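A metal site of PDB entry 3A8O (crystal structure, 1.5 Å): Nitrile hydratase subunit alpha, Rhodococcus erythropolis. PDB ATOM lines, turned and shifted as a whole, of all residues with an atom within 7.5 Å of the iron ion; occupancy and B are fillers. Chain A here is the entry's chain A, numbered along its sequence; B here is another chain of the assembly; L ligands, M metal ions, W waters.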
ATOM      1  N   GLN A  91      24.668   5.629  24.456  1.00  0.00           N
ATOM      2  CA  GLN A  91      23.364   5.034  24.761  1.00  0.00           C
ATOM      3  C   GLN A  91      22.784   5.578  26.090  1.00  0.00           C
ATOM      4  O   GLN A  91      22.008   4.924  26.781  1.00  0.00           O
ATOM      5  CB  GLN A  91      23.435   3.501  24.746  1.00  0.00           C
ATOM      6  CG  GLN A  91      23.747   2.930  23.352  1.00  0.00           C
ATOM      7  CD  GLN A  91      22.719   3.352  22.322  1.00  0.00           C
ATOM      8  OE1 GLN A  91      21.529   3.106  22.504  1.00  0.00           O
ATOM      9  NE2 GLN A  91      23.172   4.005  21.252  1.00  0.00           N
ATOM     10  N   VAL A 109      11.395  -1.664  28.202  1.00  0.00           N
ATOM     11  CA  VAL A 109      11.838  -2.712  27.258  1.00  0.00           C
ATOM     12  C   VAL A 109      12.353  -2.047  25.983  1.00  0.00           C
ATOM     13  O   VAL A 109      12.121  -0.855  25.739  1.00  0.00           O
ATOM     14  CB  VAL A 109      10.646  -3.671  26.911  1.00  0.00           C
ATOM     15  CG1 VAL A 109       9.510  -2.905  26.204  1.00  0.00           C
ATOM     16  CG2 VAL A 109      11.107  -4.876  26.077  1.00  0.00           C
ATOM     17  N   CYS A 110      13.091  -2.806  25.162  1.00  0.00           N
ATOM     18  CA  CYS A 110      13.297  -2.432  23.755  1.00  0.00           C
ATOM     19  C   CYS A 110      12.788  -3.590  22.913  1.00  0.00           C
ATOM     20  O   CYS A 110      13.514  -4.571  22.664  1.00  0.00           O
ATOM     21  CB  CYS A 110      14.768  -2.169  23.448  1.00  0.00           C
ATOM     22  SG  CYS A 110      15.062  -1.802  21.688  1.00  0.00           S
ATOM     23  N   SER A 111      11.537  -3.506  22.471  1.00  0.00           N
ATOM     24  CA  SER A 111      10.945  -4.636  21.747  1.00  0.00           C
ATOM     25  C   SER A 111      11.656  -4.929  20.427  1.00  0.00           C
ATOM     26  O   SER A 111      11.660  -6.075  19.962  1.00  0.00           O
ATOM     27  CB  SER A 111       9.440  -4.429  21.534  1.00  0.00           C
ATOM     28  OG  SER A 111       9.211  -3.447  20.560  1.00  0.00           O
ATOM     29  N   LEU A 112      12.243  -3.897  19.812  1.00  0.00           N
ATOM     30  CA  LEU A 112      12.889  -4.024  18.512  1.00  0.00           C
ATOM     31  C   LEU A 112      14.332  -4.533  18.542  1.00  0.00           C
ATOM     32  O   LEU A 112      14.850  -4.938  17.488  1.00  0.00           O
ATOM     33  CB  LEU A 112      12.770  -2.704  17.728  1.00  0.00           C
ATOM     34  CG  LEU A 112      11.359  -2.182  17.395  1.00  0.00           C
ATOM     35  CD1 LEU A 112      11.404  -0.708  16.973  1.00  0.00           C
ATOM     36  CD2 LEU A 112      10.681  -3.034  16.336  1.00  0.00           C
ATOM     37  N   CSD A 113      14.967  -4.493  19.720  1.00  0.00           N
ATOM     38  CA  CSD A 113      16.374  -4.908  19.879  1.00  0.00           C
ATOM     39  CB  CSD A 113      17.329  -4.122  18.959  1.00  0.00           C
ATOM     40  SG  CSD A 113      17.115  -2.273  19.249  1.00  0.00           S
ATOM     41  C   CSD A 113      16.808  -4.989  21.326  1.00  0.00           C
ATOM     42  O   CSD A 113      16.639  -6.065  21.932  1.00  0.00           O
ATOM     43  OD1 CSD A 113      18.342  -1.649  18.366  1.00  0.00           O
ATOM     44  OD2 CSD A 113      15.701  -1.844  18.504  1.00  0.00           O
ATOM     45  N   SER A 114      17.386  -3.933  21.907  1.00  0.00           N
ATOM     46  CA  SER A 114      17.870  -4.070  23.300  1.00  0.00           C
ATOM     47  C   SER A 114      18.127  -2.742  23.992  1.00  0.00           C
ATOM     48  O   SER A 114      18.662  -2.712  25.112  1.00  0.00           O
ATOM     49  CB  SER A 114      19.155  -4.903  23.319  1.00  0.00           C
ATOM     50  OG  SER A 114      20.191  -4.188  22.679  1.00  0.00           O
ATOM     51  N   CSO A 115      17.744  -1.669  23.321  1.00  0.00           N
ATOM     52  CA  CSO A 115      18.034  -0.318  23.788  1.00  0.00           C
ATOM     53  CB  CSO A 115      17.296   0.729  22.942  1.00  0.00           C
ATOM     54  SG  CSO A 115      17.355   0.248  21.207  1.00  0.00           S
ATOM     55  C   CSO A 115      17.792  -0.126  25.278  1.00  0.00           C
ATOM     56  O   CSO A 115      16.735  -0.469  25.813  1.00  0.00           O
ATOM     57  OD  CSO A 115      18.948   0.728  20.671  1.00  0.00           O
ATOM     58  N   THR A 116      18.831   0.417  25.918  1.00  0.00           N
ATOM     59  CA  THR A 116      19.008   0.474  27.360  1.00  0.00           C
ATOM     60  C   THR A 116      19.900   1.681  27.679  1.00  0.00           C
ATOM     61  O   THR A 116      20.835   1.974  26.929  1.00  0.00           O
ATOM     62  CB  THR A 116      19.738  -0.812  27.823  1.00  0.00           C
ATOM     63  OG1 THR A 116      18.847  -1.924  27.694  1.00  0.00           O
ATOM     64  CG2 THR A 116      20.240  -0.723  29.248  1.00  0.00           C
ATOM     65  N   PRO A 124      22.507  -4.274  28.824  1.00  0.00           N
ATOM     66  CA  PRO A 124      21.334  -5.107  29.148  1.00  0.00           C
ATOM     67  C   PRO A 124      21.725  -6.565  29.413  1.00  0.00           C
ATOM     68  O   PRO A 124      22.666  -7.089  28.793  1.00  0.00           O
ATOM     69  CB  PRO A 124      20.442  -4.988  27.902  1.00  0.00           C
ATOM     70  CG  PRO A 124      21.387  -4.625  26.782  1.00  0.00           C
ATOM     71  CD  PRO A 124      22.421  -3.706  27.467  1.00  0.00           C
ATOM     72  N   TYR A 128      16.737  -9.518  29.252  1.00  0.00           N
ATOM     73  CA  TYR A 128      16.071  -8.313  28.759  1.00  0.00           C
ATOM     74  C   TYR A 128      16.068  -8.285  27.234  1.00  0.00           C
ATOM     75  O   TYR A 128      15.142  -7.758  26.594  1.00  0.00           O
ATOM     76  CB  TYR A 128      16.767  -7.104  29.361  1.00  0.00           C
ATOM     77  CG  TYR A 128      16.326  -5.735  28.896  1.00  0.00           C
ATOM     78  CD1 TYR A 128      16.857  -5.155  27.743  1.00  0.00           C
ATOM     79  CD2 TYR A 128      15.411  -5.010  29.642  1.00  0.00           C
ATOM     80  CE1 TYR A 128      16.481  -3.872  27.328  1.00  0.00           C
ATOM     81  CE2 TYR A 128      15.021  -3.725  29.247  1.00  0.00           C
ATOM     82  CZ  TYR A 128      15.559  -3.153  28.084  1.00  0.00           C
ATOM     83  OH  TYR A 128      15.212  -1.867  27.689  1.00  0.00           O
ATOM     84  N   ARG A 134      11.023  -9.267  24.960  1.00  0.00           N
ATOM     85  CA  ARG A 134      10.701  -8.370  23.826  1.00  0.00           C
ATOM     86  C   ARG A 134       9.284  -8.559  23.268  1.00  0.00           C
ATOM     87  O   ARG A 134       8.615  -7.587  22.913  1.00  0.00           O
ATOM     88  CB  ARG A 134      11.767  -8.559  22.722  1.00  0.00           C
ATOM     89  CG  ARG A 134      13.128  -7.982  23.133  1.00  0.00           C
ATOM     90  CD  ARG A 134      14.225  -8.262  22.100  1.00  0.00           C
ATOM     91  NE  ARG A 134      13.752  -7.859  20.785  1.00  0.00           N
ATOM     92  CZ  ARG A 134      14.276  -8.269  19.632  1.00  0.00           C
ATOM     93  NH1 ARG A 134      15.313  -9.077  19.590  1.00  0.00           N
ATOM     94  NH2 ARG A 134      13.742  -7.854  18.488  1.00  0.00           N
ATOM     95  N   ASP A 162       8.418   1.424  25.676  1.00  0.00           N
ATOM     96  CA  ASP A 162       9.187   0.759  24.622  1.00  0.00           C
ATOM     97  C   ASP A 162      10.214   1.750  24.089  1.00  0.00           C
ATOM     98  O   ASP A 162       9.854   2.836  23.577  1.00  0.00           O
ATOM     99  CB  ASP A 162       8.241   0.301  23.497  1.00  0.00           C
ATOM    100  CG  ASP A 162       8.848  -0.773  22.615  1.00  0.00           C
ATOM    101  OD1 ASP A 162      10.090  -1.040  22.667  1.00  0.00           O
ATOM    102  OD2 ASP A 162       8.077  -1.344  21.825  1.00  0.00           O
ATOM    103  N   THR A 163      11.494   1.383  24.193  1.00  0.00           N
ATOM    104  CA  THR A 163      12.610   2.246  23.886  1.00  0.00           C
ATOM    105  C   THR A 163      12.899   2.175  22.381  1.00  0.00           C
ATOM    106  O   THR A 163      13.760   1.428  21.931  1.00  0.00           O
ATOM    107  CB  THR A 163      13.861   1.860  24.708  1.00  0.00           C
ATOM    108  OG1 THR A 163      13.516   1.789  26.100  1.00  0.00           O
ATOM    109  CG2 THR A 163      14.948   2.881  24.534  1.00  0.00           C
ATOM    110  N   THR A 164      12.151   2.961  21.617  1.00  0.00           N
ATOM    111  CA  THR A 164      12.130   2.846  20.150  1.00  0.00           C
ATOM    112  C   THR A 164      12.920   3.945  19.425  1.00  0.00           C
ATOM    113  O   THR A 164      13.028   3.933  18.197  1.00  0.00           O
ATOM    114  CB  THR A 164      10.696   2.859  19.618  1.00  0.00           C
ATOM    115  OG1 THR A 164       9.994   3.937  20.258  1.00  0.00           O
ATOM    116  CG2 THR A 164       9.975   1.556  19.954  1.00  0.00           C
ATOM    117  N   ALA A 165      13.445   4.934  20.166  1.00  0.00           N
ATOM    118  CA  ALA A 165      14.236   6.001  19.526  1.00  0.00           C
ATOM    119  C   ALA A 165      15.464   6.331  20.381  1.00  0.00           C
ATOM    120  O   ALA A 165      16.216   5.416  20.728  1.00  0.00           O
ATOM    121  CB  ALA A 165      13.367   7.223  19.254  1.00  0.00           C
ATOM    122  N   ARG A 168      16.497   7.404  26.548  1.00  0.00           N
ATOM    123  CA  ARG A 168      16.981   6.288  27.335  1.00  0.00           C
ATOM    124  C   ARG A 168      16.420   6.458  28.739  1.00  0.00           C
ATOM    125  O   ARG A 168      16.582   7.506  29.366  1.00  0.00           O
ATOM    126  CB  ARG A 168      18.523   6.236  27.297  1.00  0.00           C
ATOM    127  CG  ARG A 168      19.064   5.947  25.907  1.00  0.00           C
ATOM    128  CD  ARG A 168      18.868   4.471  25.504  1.00  0.00           C
ATOM    129  NE  ARG A 168      19.296   4.223  24.120  1.00  0.00           N
ATOM    130  CZ  ARG A 168      18.539   4.445  23.052  1.00  0.00           C
ATOM    131  NH1 ARG A 168      17.296   4.891  23.190  1.00  0.00           N
ATOM    132  NH2 ARG A 168      19.031   4.212  21.837  1.00  0.00           N
ATOM    133  N   ARG B  56      21.417  -1.247  13.384  1.00  0.00           N
ATOM    134  CA  ARG B  56      20.098  -1.814  13.686  1.00  0.00           C
ATOM    135  C   ARG B  56      19.507  -2.454  12.430  1.00  0.00           C
ATOM    136  O   ARG B  56      19.015  -3.595  12.482  1.00  0.00           O
ATOM    137  CB  ARG B  56      19.134  -0.746  14.220  1.00  0.00           C
ATOM    138  CG  ARG B  56      19.529  -0.184  15.568  1.00  0.00           C
ATOM    139  CD  ARG B  56      18.373   0.556  16.234  1.00  0.00           C
ATOM    140  NE  ARG B  56      18.818   1.077  17.526  1.00  0.00           N
ATOM    141  CZ  ARG B  56      19.411   2.261  17.699  1.00  0.00           C
ATOM    142  NH1 ARG B  56      19.587   3.093  16.669  1.00  0.00           N
ATOM    143  NH2 ARG B  56      19.815   2.628  18.910  1.00  0.00           N
ATOM    144  N   TYR B  72      22.058 -13.038  20.849  1.00  0.00           N
ATOM    145  CA  TYR B  72      22.185 -11.603  20.734  1.00  0.00           C
ATOM    146  C   TYR B  72      23.545 -11.089  20.226  1.00  0.00           C
ATOM    147  O   TYR B  72      23.609 -10.415  19.196  1.00  0.00           O
ATOM    148  CB  TYR B  72      21.837 -10.947  22.077  1.00  0.00           C
ATOM    149  CG  TYR B  72      21.978  -9.461  22.036  1.00  0.00           C
ATOM    150  CD1 TYR B  72      20.915  -8.659  21.616  1.00  0.00           C
ATOM    151  CD2 TYR B  72      23.189  -8.832  22.362  1.00  0.00           C
ATOM    152  CE1 TYR B  72      21.030  -7.290  21.549  1.00  0.00           C
ATOM    153  CE2 TYR B  72      23.317  -7.435  22.291  1.00  0.00           C
ATOM    154  CZ  TYR B  72      22.227  -6.675  21.886  1.00  0.00           C
ATOM    155  OH  TYR B  72      22.334  -5.300  21.818  1.00  0.00           O
ATOM    156  N   TYR B  76      25.194  -9.176  16.241  1.00  0.00           N
ATOM    157  CA  TYR B  76      25.966  -7.952  16.014  1.00  0.00           C
ATOM    158  C   TYR B  76      27.328  -8.214  15.389  1.00  0.00           C
ATOM    159  O   TYR B  76      27.818  -7.387  14.630  1.00  0.00           O
ATOM    160  CB  TYR B  76      26.002  -7.049  17.284  1.00  0.00           C
ATOM    161  CG  TYR B  76      24.599  -6.578  17.582  1.00  0.00           C
ATOM    162  CD1 TYR B  76      24.081  -5.418  16.992  1.00  0.00           C
ATOM    163  CD2 TYR B  76      23.741  -7.371  18.321  1.00  0.00           C
ATOM    164  CE1 TYR B  76      22.756  -5.033  17.228  1.00  0.00           C
ATOM    165  CE2 TYR B  76      22.423  -7.007  18.550  1.00  0.00           C
ATOM    166  CZ  TYR B  76      21.926  -5.835  17.998  1.00  0.00           C
ATOM    167  OH  TYR B  76      20.616  -5.506  18.232  1.00  0.00           O
ATOM    168  N   ARG B 141      11.571   2.978  12.876  1.00  0.00           N
ATOM    169  CA  ARG B 141      11.503   2.841  14.334  1.00  0.00           C
ATOM    170  C   ARG B 141      10.086   2.905  14.862  1.00  0.00           C
ATOM    171  O   ARG B 141       9.799   3.505  15.910  1.00  0.00           O
ATOM    172  CB  ARG B 141      12.408   3.871  15.016  1.00  0.00           C
ATOM    173  CG  ARG B 141      13.887   3.598  14.754  1.00  0.00           C
ATOM    174  CD  ARG B 141      14.244   2.143  15.100  1.00  0.00           C
ATOM    175  NE  ARG B 141      14.291   1.919  16.537  1.00  0.00           N
ATOM    176  CZ  ARG B 141      14.638   0.784  17.115  1.00  0.00           C
ATOM    177  NH1 ARG B 141      14.935  -0.291  16.377  1.00  0.00           N
ATOM    178  NH2 ARG B 141      14.716   0.725  18.432  1.00  0.00           N
HETATM  179  C1  LIG L   1      24.339  -1.147  19.038  1.00  0.00           C
HETATM  180  C2  LIG L   1      21.959  -0.777  18.460  1.00  0.00           C
HETATM  181  C3  LIG L   1      22.898   0.337  20.472  1.00  0.00           C
HETATM  182  N1  LIG L   1      22.120  -3.191  19.800  1.00  0.00           N
HETATM  183  O1  LIG L   1      22.918  -2.215  21.629  1.00  0.00           O
HETATM  184  C4  LIG L   1      22.657  -2.158  20.435  1.00  0.00           C
HETATM  185  C5  LIG L   1      22.949  -0.922  19.607  1.00  0.00           C
HETATM  186 FE    FE M   1      17.374  -1.939  21.382  1.00  0.00          FE
HETATM  187  O   HOH W   1      19.238  -2.055  21.007  1.00  0.00           O
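The side-chain hydroxyl of Tyr 76 of chain B lies within hydrogen-bond range of a nitrogen (N1) of the ligand, at 3.2 Å. OH of Tyr 72 of chain B is in hydrogen-bond range of N1 of the ligand (2.9 Å).
OD of CSO 115 is in hydrogen-bond range of NH2 of Arg 56 of chain B, at 2.7 Å. OH of Tyr 128 lies within hydrogen-bond range of O of CSO 115 (2.8 Å). The backbone carbonyl oxygen (O) of Ser 114 sits at hydrogen-bond distance from the side-chain hydroxyl (OG1) of Thr 116. OG of Ser 114 is in hydrogen-bond range of OH of Tyr 72 of chain B, 2.6 Å away. NH1 of Arg 141 of chain B is in salt-bridge range of OD2 of CSD 113 (2.7 Å). NE of Arg 56 of chain B is in salt-bridge range of OD1 of CSD 113, 2.9 Å away. SG of Cys 110 lies close to O of Thr 163 (3.5 Å). The backbone NH (N) of Cys 110 lies within hydrogen-bond range of the side-chain hydroxyl (OH) of Tyr 128, at 3.4 Å.
Of the 21 residues printed, 4 come within 4 Å of the iron ion.
The iron ion is bound by water W1 (1.9 Å), N of CSO 115 (2.0 Å), the backbone nitrogen of Ser 114 (2.1 Å), SG of CSD 113 (2.2 Å), SG of CSO 115 (2.2 Å) and the side-chain sulfur of Cys 110 (2.3 Å). The iron ion has six donor atoms within binding distance.
Water W1 lies within hydrogen-bond range of OD1 of CSD 113 (2.8 Å), OD of CSO 115 (2.8 Å), OG of Ser 114 (2.9 Å) and N1 of the ligand (3.3 Å).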
